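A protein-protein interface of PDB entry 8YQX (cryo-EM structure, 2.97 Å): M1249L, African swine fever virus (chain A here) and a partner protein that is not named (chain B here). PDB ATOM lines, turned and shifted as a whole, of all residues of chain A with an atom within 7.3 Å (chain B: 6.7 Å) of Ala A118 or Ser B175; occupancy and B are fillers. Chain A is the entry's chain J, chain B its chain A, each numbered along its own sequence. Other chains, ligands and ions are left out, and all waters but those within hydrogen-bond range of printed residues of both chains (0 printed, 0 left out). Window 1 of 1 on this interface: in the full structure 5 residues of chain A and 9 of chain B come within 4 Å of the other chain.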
ATOM      1  N   ARG A 106      -0.733  -5.697  30.511  1.00  0.00           N
ATOM      2  CA  ARG A 106      -1.477  -6.932  30.719  1.00  0.00           C
ATOM      3  C   ARG A 106      -0.532  -8.035  31.175  1.00  0.00           C
ATOM      4  O   ARG A 106       0.583  -8.175  30.664  1.00  0.00           O
ATOM      5  CB  ARG A 106      -2.214  -7.343  29.442  1.00  0.00           C
ATOM      6  CG  ARG A 106      -1.320  -7.756  28.288  1.00  0.00           C
ATOM      7  CD  ARG A 106      -2.122  -8.418  27.182  1.00  0.00           C
ATOM      8  NE  ARG A 106      -2.687  -9.694  27.604  1.00  0.00           N
ATOM      9  CZ  ARG A 106      -2.009 -10.832  27.665  1.00  0.00           C
ATOM     10  NH1 ARG A 106      -0.727 -10.890  27.345  1.00  0.00           N
ATOM     11  NH2 ARG A 106      -2.633 -11.938  28.056  1.00  0.00           N
ATOM     12  N   LYS A 107      -0.969  -8.805  32.168  1.00  0.00           N
ATOM     13  CA  LYS A 107      -0.109  -9.807  32.782  1.00  0.00           C
ATOM     14  C   LYS A 107      -0.882 -11.102  32.958  1.00  0.00           C
ATOM     15  O   LYS A 107      -2.021 -11.086  33.428  1.00  0.00           O
ATOM     16  CB  LYS A 107       0.425  -9.322  34.134  1.00  0.00           C
ATOM     17  CG  LYS A 107       1.393 -10.282  34.801  1.00  0.00           C
ATOM     18  CD  LYS A 107       2.693 -10.391  34.022  1.00  0.00           C
ATOM     19  CE  LYS A 107       3.728 -11.201  34.786  1.00  0.00           C
ATOM     20  NZ  LYS A 107       4.993 -11.358  34.017  1.00  0.00           N
ATOM     21  N   GLU A 108      -0.265 -12.217  32.581  1.00  0.00           N
ATOM     22  CA  GLU A 108      -0.856 -13.532  32.786  1.00  0.00           C
ATOM     23  C   GLU A 108      -0.451 -14.037  34.163  1.00  0.00           C
ATOM     24  O   GLU A 108       0.743 -14.159  34.458  1.00  0.00           O
ATOM     25  CB  GLU A 108      -0.410 -14.497  31.692  1.00  0.00           C
ATOM     26  CG  GLU A 108      -0.539 -13.923  30.294  1.00  0.00           C
ATOM     27  CD  GLU A 108      -0.446 -14.979  29.214  1.00  0.00           C
ATOM     28  OE1 GLU A 108      -0.548 -16.179  29.537  1.00  0.00           O
ATOM     29  OE2 GLU A 108      -0.271 -14.606  28.037  1.00  0.00           O
ATOM     30  N   ILE A 109      -1.441 -14.325  35.006  1.00  0.00           N
ATOM     31  CA  ILE A 109      -1.225 -14.699  36.393  1.00  0.00           C
ATOM     32  C   ILE A 109      -1.957 -16.005  36.669  1.00  0.00           C
ATOM     33  O   ILE A 109      -2.760 -16.485  35.865  1.00  0.00           O
ATOM     34  CB  ILE A 109      -1.697 -13.604  37.373  1.00  0.00           C
ATOM     35  CG1 ILE A 109      -3.168 -13.267  37.127  1.00  0.00           C
ATOM     36  CG2 ILE A 109      -0.845 -12.358  37.228  1.00  0.00           C
ATOM     37  CD1 ILE A 109      -3.981 -13.118  38.393  1.00  0.00           C
ATOM     38  N   PHE A 110      -1.651 -16.583  37.824  1.00  0.00           N
ATOM     39  CA  PHE A 110      -2.287 -17.795  38.307  1.00  0.00           C
ATOM     40  C   PHE A 110      -3.040 -17.495  39.595  1.00  0.00           C
ATOM     41  O   PHE A 110      -2.907 -16.421  40.185  1.00  0.00           O
ATOM     42  CB  PHE A 110      -1.261 -18.906  38.561  1.00  0.00           C
ATOM     43  CG  PHE A 110      -0.456 -19.282  37.351  1.00  0.00           C
ATOM     44  CD1 PHE A 110      -1.023 -20.015  36.325  1.00  0.00           C
ATOM     45  CD2 PHE A 110       0.871 -18.904  37.245  1.00  0.00           C
ATOM     46  CE1 PHE A 110      -0.282 -20.362  35.214  1.00  0.00           C
ATOM     47  CE2 PHE A 110       1.616 -19.248  36.135  1.00  0.00           C
ATOM     48  CZ  PHE A 110       1.039 -19.977  35.119  1.00  0.00           C
ATOM     49  N   LEU A 111      -3.844 -18.462  40.017  1.00  0.00           N
ATOM     50  CA  LEU A 111      -4.535 -18.417  41.293  1.00  0.00           C
ATOM     51  C   LEU A 111      -4.326 -19.738  42.019  1.00  0.00           C
ATOM     52  O   LEU A 111      -3.987 -20.756  41.409  1.00  0.00           O
ATOM     53  CB  LEU A 111      -6.034 -18.137  41.115  1.00  0.00           C
ATOM     54  CG  LEU A 111      -6.441 -16.842  40.407  1.00  0.00           C
ATOM     55  CD1 LEU A 111      -6.607 -17.037  38.910  1.00  0.00           C
ATOM     56  CD2 LEU A 111      -7.717 -16.286  41.016  1.00  0.00           C
ATOM     57  N   THR A 115      -5.288 -21.925  38.215  1.00  0.00           N
ATOM     58  CA  THR A 115      -6.039 -21.516  37.035  1.00  0.00           C
ATOM     59  C   THR A 115      -5.363 -20.300  36.417  1.00  0.00           C
ATOM     60  O   THR A 115      -5.036 -19.339  37.121  1.00  0.00           O
ATOM     61  CB  THR A 115      -7.505 -21.219  37.378  1.00  0.00           C
ATOM     62  OG1 THR A 115      -8.132 -22.399  37.901  1.00  0.00           O
ATOM     63  CG2 THR A 115      -8.264 -20.718  36.162  1.00  0.00           C
ATOM     64  N   HIS A 116      -5.149 -20.352  35.105  1.00  0.00           N
ATOM     65  CA  HIS A 116      -4.369 -19.347  34.390  1.00  0.00           C
ATOM     66  C   HIS A 116      -5.313 -18.301  33.809  1.00  0.00           C
ATOM     67  O   HIS A 116      -6.154 -18.619  32.963  1.00  0.00           O
ATOM     68  CB  HIS A 116      -3.542 -20.010  33.293  1.00  0.00           C
ATOM     69  CG  HIS A 116      -2.414 -19.167  32.788  1.00  0.00           C
ATOM     70  ND1 HIS A 116      -1.819 -19.380  31.563  1.00  0.00           N
ATOM     71  CD2 HIS A 116      -1.771 -18.110  33.339  1.00  0.00           C
ATOM     72  CE1 HIS A 116      -0.857 -18.494  31.384  1.00  0.00           C
ATOM     73  NE2 HIS A 116      -0.808 -17.712  32.447  1.00  0.00           N
ATOM     74  N   LEU A 117      -5.173 -17.052  34.256  1.00  0.00           N
ATOM     75  CA  LEU A 117      -6.008 -15.968  33.760  1.00  0.00           C
ATOM     76  C   LEU A 117      -5.151 -14.734  33.534  1.00  0.00           C
ATOM     77  O   LEU A 117      -4.188 -14.492  34.259  1.00  0.00           O
ATOM     78  CB  LEU A 117      -7.148 -15.639  34.733  1.00  0.00           C
ATOM     79  CG  LEU A 117      -8.213 -16.716  34.944  1.00  0.00           C
ATOM     80  CD1 LEU A 117      -9.069 -16.382  36.150  1.00  0.00           C
ATOM     81  CD2 LEU A 117      -9.072 -16.871  33.702  1.00  0.00           C
ATOM     82  N   ALA A 118      -5.512 -13.949  32.528  1.00  0.00           N
ATOM     83  CA  ALA A 118      -4.811 -12.702  32.272  1.00  0.00           C
ATOM     84  C   ALA A 118      -5.538 -11.538  32.935  1.00  0.00           C
ATOM     85  O   ALA A 118      -6.720 -11.623  33.275  1.00  0.00           O
ATOM     86  CB  ALA A 118      -4.674 -12.454  30.771  1.00  0.00           C
ATOM     87  N   VAL A 119      -4.806 -10.447  33.135  1.00  0.00           N
ATOM     88  CA  VAL A 119      -5.378  -9.214  33.667  1.00  0.00           C
ATOM     89  C   VAL A 119      -4.928  -8.055  32.785  1.00  0.00           C
ATOM     90  O   VAL A 119      -3.824  -8.098  32.218  1.00  0.00           O
ATOM     91  CB  VAL A 119      -4.981  -8.988  35.135  1.00  0.00           C
ATOM     92  CG1 VAL A 119      -5.552 -10.082  36.021  1.00  0.00           C
ATOM     93  CG2 VAL A 119      -3.473  -8.905  35.281  1.00  0.00           C
ATOM     94  N   PRO A 120      -5.739  -7.003  32.647  1.00  0.00           N
ATOM     95  CA  PRO A 120      -5.357  -5.880  31.779  1.00  0.00           C
ATOM     96  C   PRO A 120      -4.250  -5.024  32.373  1.00  0.00           C
ATOM     97  O   PRO A 120      -3.688  -5.354  33.421  1.00  0.00           O
ATOM     98  CB  PRO A 120      -6.663  -5.089  31.635  1.00  0.00           C
ATOM     99  CG  PRO A 120      -7.459  -5.450  32.840  1.00  0.00           C
ATOM    100  CD  PRO A 120      -7.118  -6.874  33.145  1.00  0.00           C
ATOM    101  N   ALA A 121      -3.938  -3.912  31.703  1.00  0.00           N
ATOM    102  CA  ALA A 121      -2.807  -3.069  32.076  1.00  0.00           C
ATOM    103  C   ALA A 121      -2.952  -2.428  33.450  1.00  0.00           C
ATOM    104  O   ALA A 121      -2.016  -1.761  33.899  1.00  0.00           O
ATOM    105  CB  ALA A 121      -2.601  -1.979  31.023  1.00  0.00           C
ATOM    106  N   GLU A 122      -4.089  -2.600  34.121  1.00  0.00           N
ATOM    107  CA  GLU A 122      -4.255  -2.067  35.471  1.00  0.00           C
ATOM    108  C   GLU A 122      -5.353  -2.867  36.156  1.00  0.00           C
ATOM    109  O   GLU A 122      -6.522  -2.769  35.771  1.00  0.00           O
ATOM    110  CB  GLU A 122      -4.592  -0.582  35.434  1.00  0.00           C
ATOM    111  CG  GLU A 122      -4.208   0.169  36.697  1.00  0.00           C
ATOM    112  CD  GLU A 122      -2.728   0.497  36.751  1.00  0.00           C
ATOM    113  OE1 GLU A 122      -2.104   0.613  35.676  1.00  0.00           O
ATOM    114  OE2 GLU A 122      -2.191   0.637  37.869  1.00  0.00           O
ATOM    115  N   ALA A 123      -4.979  -3.650  37.160  1.00  0.00           N
ATOM    116  CA  ALA A 123      -5.936  -4.454  37.906  1.00  0.00           C
ATOM    117  C   ALA A 123      -5.365  -4.785  39.278  1.00  0.00           C
ATOM    118  O   ALA A 123      -4.271  -5.355  39.373  1.00  0.00           O
ATOM    119  CB  ALA A 123      -6.279  -5.734  37.144  1.00  0.00           C
ATOM    120  N   CYS B 102     -13.805 -12.458  32.672  1.00  0.00           N
ATOM    121  CA  CYS B 102     -12.486 -12.883  33.114  1.00  0.00           C
ATOM    122  C   CYS B 102     -11.556 -13.288  31.981  1.00  0.00           C
ATOM    123  O   CYS B 102     -10.358 -13.462  32.228  1.00  0.00           O
ATOM    124  CB  CYS B 102     -12.598 -14.055  34.101  1.00  0.00           C
ATOM    125  SG  CYS B 102     -13.141 -15.603  33.356  1.00  0.00           S
ATOM    126  N   GLY B 103     -12.057 -13.442  30.757  1.00  0.00           N
ATOM    127  CA  GLY B 103     -11.237 -13.805  29.626  1.00  0.00           C
ATOM    128  C   GLY B 103     -11.086 -15.291  29.388  1.00  0.00           C
ATOM    129  O   GLY B 103     -10.520 -15.680  28.359  1.00  0.00           O
ATOM    130  N   ILE B 170     -13.972  -3.472  24.404  1.00  0.00           N
ATOM    131  CA  ILE B 170     -13.521  -4.639  23.652  1.00  0.00           C
ATOM    132  C   ILE B 170     -12.037  -4.883  23.888  1.00  0.00           C
ATOM    133  O   ILE B 170     -11.597  -6.030  24.030  1.00  0.00           O
ATOM    134  CB  ILE B 170     -13.836  -4.463  22.155  1.00  0.00           C
ATOM    135  CG1 ILE B 170     -15.341  -4.327  21.938  1.00  0.00           C
ATOM    136  CG2 ILE B 170     -13.300  -5.633  21.359  1.00  0.00           C
ATOM    137  CD1 ILE B 170     -15.720  -4.028  20.511  1.00  0.00           C
ATOM    138  N   ARG B 171     -11.240  -3.813  23.927  1.00  0.00           N
ATOM    139  CA  ARG B 171      -9.810  -3.958  24.176  1.00  0.00           C
ATOM    140  C   ARG B 171      -9.545  -4.500  25.575  1.00  0.00           C
ATOM    141  O   ARG B 171      -8.666  -5.348  25.763  1.00  0.00           O
ATOM    142  CB  ARG B 171      -9.105  -2.617  23.966  1.00  0.00           C
ATOM    143  CG  ARG B 171      -8.090  -2.251  25.038  1.00  0.00           C
ATOM    144  CD  ARG B 171      -6.991  -1.368  24.477  1.00  0.00           C
ATOM    145  NE  ARG B 171      -6.213  -2.055  23.454  1.00  0.00           N
ATOM    146  CZ  ARG B 171      -5.197  -1.512  22.796  1.00  0.00           C
ATOM    147  NH1 ARG B 171      -4.810  -0.268  23.026  1.00  0.00           N
ATOM    148  NH2 ARG B 171      -4.555  -2.236  21.884  1.00  0.00           N
ATOM    149  N   GLU B 172     -10.295  -4.021  26.571  1.00  0.00           N
ATOM    150  CA  GLU B 172     -10.137  -4.541  27.926  1.00  0.00           C
ATOM    151  C   GLU B 172     -10.525  -6.012  27.998  1.00  0.00           C
ATOM    152  O   GLU B 172      -9.883  -6.797  28.704  1.00  0.00           O
ATOM    153  CB  GLU B 172     -10.970  -3.720  28.910  1.00  0.00           C
ATOM    154  CG  GLU B 172     -10.582  -3.926  30.364  1.00  0.00           C
ATOM    155  CD  GLU B 172      -9.938  -2.702  30.978  1.00  0.00           C
ATOM    156  OE1 GLU B 172      -9.408  -1.864  30.219  1.00  0.00           O
ATOM    157  OE2 GLU B 172      -9.960  -2.577  32.220  1.00  0.00           O
ATOM    158  N   ILE B 173     -11.581  -6.398  27.283  1.00  0.00           N
ATOM    159  CA  ILE B 173     -11.990  -7.799  27.246  1.00  0.00           C
ATOM    160  C   ILE B 173     -10.914  -8.654  26.586  1.00  0.00           C
ATOM    161  O   ILE B 173     -10.594  -9.750  27.062  1.00  0.00           O
ATOM    162  CB  ILE B 173     -13.344  -7.931  26.526  1.00  0.00           C
ATOM    163  CG1 ILE B 173     -14.481  -7.459  27.432  1.00  0.00           C
ATOM    164  CG2 ILE B 173     -13.581  -9.357  26.083  1.00  0.00           C
ATOM    165  CD1 ILE B 173     -15.769  -7.183  26.694  1.00  0.00           C
ATOM    166  N   PHE B 174     -10.335  -8.167  25.486  1.00  0.00           N
ATOM    167  CA  PHE B 174      -9.375  -8.960  24.726  1.00  0.00           C
ATOM    168  C   PHE B 174      -8.027  -9.059  25.429  1.00  0.00           C
ATOM    169  O   PHE B 174      -7.341 -10.078  25.300  1.00  0.00           O
ATOM    170  CB  PHE B 174      -9.197  -8.367  23.331  1.00  0.00           C
ATOM    171  CG  PHE B 174     -10.282  -8.748  22.370  1.00  0.00           C
ATOM    172  CD1 PHE B 174     -11.161  -9.771  22.671  1.00  0.00           C
ATOM    173  CD2 PHE B 174     -10.421  -8.083  21.166  1.00  0.00           C
ATOM    174  CE1 PHE B 174     -12.159 -10.121  21.792  1.00  0.00           C
ATOM    175  CE2 PHE B 174     -11.418  -8.433  20.282  1.00  0.00           C
ATOM    176  CZ  PHE B 174     -12.287  -9.452  20.597  1.00  0.00           C
ATOM    177  N   SER B 175      -7.626  -8.022  26.165  1.00  0.00           N
ATOM    178  CA  SER B 175      -6.364  -8.071  26.893  1.00  0.00           C
ATOM    179  C   SER B 175      -6.395  -9.066  28.043  1.00  0.00           C
ATOM    180  O   SER B 175      -5.339  -9.367  28.608  1.00  0.00           O
ATOM    181  CB  SER B 175      -6.008  -6.682  27.422  1.00  0.00           C
ATOM    182  OG  SER B 175      -6.713  -6.395  28.616  1.00  0.00           O
ATOM    183  N   ARG B 176      -7.569  -9.576  28.396  1.00  0.00           N
ATOM    184  CA  ARG B 176      -7.725 -10.568  29.448  1.00  0.00           C
ATOM    185  C   ARG B 176      -7.616 -11.993  28.923  1.00  0.00           C
ATOM    186  O   ARG B 176      -7.810 -12.940  29.690  1.00  0.00           O
ATOM    187  CB  ARG B 176      -9.070 -10.365  30.150  1.00  0.00           C
ATOM    188  CG  ARG B 176      -8.969 -10.201  31.651  1.00  0.00           C
ATOM    189  CD  ARG B 176     -10.336 -10.027  32.285  1.00  0.00           C
ATOM    190  NE  ARG B 176     -10.848  -8.671  32.129  1.00  0.00           N
ATOM    191  CZ  ARG B 176     -11.956  -8.361  31.472  1.00  0.00           C
ATOM    192  NH1 ARG B 176     -12.689  -9.285  30.875  1.00  0.00           N
ATOM    193  NH2 ARG B 176     -12.339  -7.089  31.411  1.00  0.00           N
ATOM    194  N   VAL B 177      -7.311 -12.161  27.639  1.00  0.00           N
ATOM    195  CA  VAL B 177      -7.180 -13.471  27.010  1.00  0.00           C
ATOM    196  C   VAL B 177      -5.721 -13.896  27.076  1.00  0.00           C
ATOM    197  O   VAL B 177      -4.825 -13.132  26.698  1.00  0.00           O
ATOM    198  CB  VAL B 177      -7.673 -13.440  25.553  1.00  0.00           C
ATOM    199  CG1 VAL B 177      -7.590 -14.821  24.934  1.00  0.00           C
ATOM    200  CG2 VAL B 177      -9.088 -12.907  25.485  1.00  0.00           C
ATOM    201  N   THR B 178      -5.479 -15.112  27.556  1.00  0.00           N
ATOM    202  CA  THR B 178      -4.124 -15.628  27.644  1.00  0.00           C
ATOM    203  C   THR B 178      -3.678 -16.192  26.299  1.00  0.00           C
ATOM    204  O   THR B 178      -4.489 -16.503  25.424  1.00  0.00           O
ATOM    205  CB  THR B 178      -4.026 -16.707  28.721  1.00  0.00           C
ATOM    206  OG1 THR B 178      -4.995 -17.729  28.466  1.00  0.00           O
ATOM    207  CG2 THR B 178      -4.279 -16.109  30.094  1.00  0.00           C
ATOM    208  N   TYR B 179      -2.357 -16.319  26.138  1.00  0.00           N
ATOM    209  CA  TYR B 179      -1.811 -16.899  24.917  1.00  0.00           C
ATOM    210  C   TYR B 179      -2.121 -18.383  24.794  1.00  0.00           C
ATOM    211  O   TYR B 179      -2.120 -18.912  23.678  1.00  0.00           O
ATOM    212  CB  TYR B 179      -0.299 -16.682  24.850  1.00  0.00           C
ATOM    213  CG  TYR B 179       0.102 -15.338  24.293  1.00  0.00           C
ATOM    214  CD1 TYR B 179       0.065 -15.091  22.929  1.00  0.00           C
ATOM    215  CD2 TYR B 179       0.523 -14.316  25.129  1.00  0.00           C
ATOM    216  CE1 TYR B 179       0.431 -13.866  22.418  1.00  0.00           C
ATOM    217  CE2 TYR B 179       0.890 -13.088  24.627  1.00  0.00           C
ATOM    218  CZ  TYR B 179       0.844 -12.867  23.270  1.00  0.00           C
ATOM    219  OH  TYR B 179       1.211 -11.642  22.765  1.00  0.00           O
ATOM    220  N   HIS B 192      -2.819 -12.445  18.537  1.00  0.00           N
ATOM    221  CA  HIS B 192      -3.574 -12.260  19.765  1.00  0.00           C
ATOM    222  C   HIS B 192      -4.680 -11.232  19.535  1.00  0.00           C
ATOM    223  O   HIS B 192      -4.470 -10.245  18.824  1.00  0.00           O
ATOM    224  CB  HIS B 192      -2.652 -11.799  20.892  1.00  0.00           C
ATOM    225  CG  HIS B 192      -3.211 -12.014  22.265  1.00  0.00           C
ATOM    226  ND1 HIS B 192      -4.058 -11.115  22.874  1.00  0.00           N
ATOM    227  CD2 HIS B 192      -3.037 -13.024  23.149  1.00  0.00           C
ATOM    228  CE1 HIS B 192      -4.385 -11.562  24.072  1.00  0.00           C
ATOM    229  NE2 HIS B 192      -3.779 -12.719  24.263  1.00  0.00           N
ATOM    230  N   PRO B 193      -5.866 -11.437  20.111  1.00  0.00           N
ATOM    231  CA  PRO B 193      -6.971 -10.498  19.866  1.00  0.00           C
ATOM    232  C   PRO B 193      -6.709  -9.084  20.359  1.00  0.00           C
ATOM    233  O   PRO B 193      -7.375  -8.154  19.890  1.00  0.00           O
ATOM    234  CB  PRO B 193      -8.149 -11.141  20.610  1.00  0.00           C
ATOM    235  CG  PRO B 193      -7.519 -12.047  21.607  1.00  0.00           C
ATOM    236  CD  PRO B 193      -6.295 -12.576  20.935  1.00  0.00           C
ATOM    237  N   GLU B 194      -5.763  -8.885  21.280  1.00  0.00           N
ATOM    238  CA  GLU B 194      -5.493  -7.542  21.784  1.00  0.00           C
ATOM    239  C   GLU B 194      -4.985  -6.610  20.694  1.00  0.00           C
ATOM    240  O   GLU B 194      -5.058  -5.388  20.855  1.00  0.00           O
ATOM    241  CB  GLU B 194      -4.481  -7.596  22.929  1.00  0.00           C
ATOM    242  CG  GLU B 194      -3.085  -8.025  22.509  1.00  0.00           C
ATOM    243  CD  GLU B 194      -2.083  -6.890  22.568  1.00  0.00           C
ATOM    244  OE1 GLU B 194      -1.078  -6.942  21.829  1.00  0.00           O
ATOM    245  OE2 GLU B 194      -2.297  -5.948  23.359  1.00  0.00           O
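N of Tyr B179 lies close to OE2 of Glu A108, at 3.3 Å. O of Val B177 lies within hydrogen-bond range of NH2 of Arg A106 (2.8 Å). The backbone carbonyl oxygen (O) of Ser B175 sits at hydrogen-bond distance from the guanidinium group (NE) of Arg A106 (2.9 Å).
NH2 of Arg A106 is in salt-bridge range of OE2 of Glu A108, 3.6 Å away. The side-chain hydroxyl (OG) of Ser B175 sits at hydrogen-bond distance from the backbone carbonyl oxygen (O) of Glu B172. N of Ile A109 is in hydrogen-bond range of O of Leu A117 (2.9 Å). NE2 of His B192 sits at hydrogen-bond distance from O of Val B177, at 2.7 Å. The side-chain carboxylate (OE1) of Glu A108 sits close to a ring nitrogen (NE2) of His A116, at 3.3 Å.
CE2 of Tyr B179 touches NH1 of Arg A106, at 3.9 Å. Thr B178 touches Glu A108. Leu A117 touches Cys B102. Leu A117 touches Thr B178. Ser B175 touches Ala A118 (O to CB, 3.8 Å). Arg B176 touches Ala A118. CG2 of Thr B178 touches N of Ala A118, at 3.5 Å. Glu B172 touches Pro A120 (OE2 to CG, 3.9 Å). Pro A120 touches Ser B175.
Of chain A, only Arg A106, Ala A118 and Pro A120 come within 4 Å of Ser B175. Printed residues of chain A within 4 Å of Val B177: Arg A106. Printed residues of chain B within 4 Å of Leu A117: Cys B102 (3.9 Å) and Thr B178 (3.8 Å). Printed residues of chain A within 4 Å of Cys B102: Leu A117. Of the printed residues of chain A, Arg B176 touches Ala A118. Gly B103 touches none of the printed residues of chain A. The nearest residue of chain B that does not touch Ala A118 is Val B177 (4.1 Å). The nearest printed residue of chain A that does not touch Arg B176 is Pro A120 (4.1 Å).
Of the 15 printed residues of chain B, 7 touch a printed residue of chain A. Hydrophobic or aromatic side chains of chain B that line the printed part of chain A: Tyr B179.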
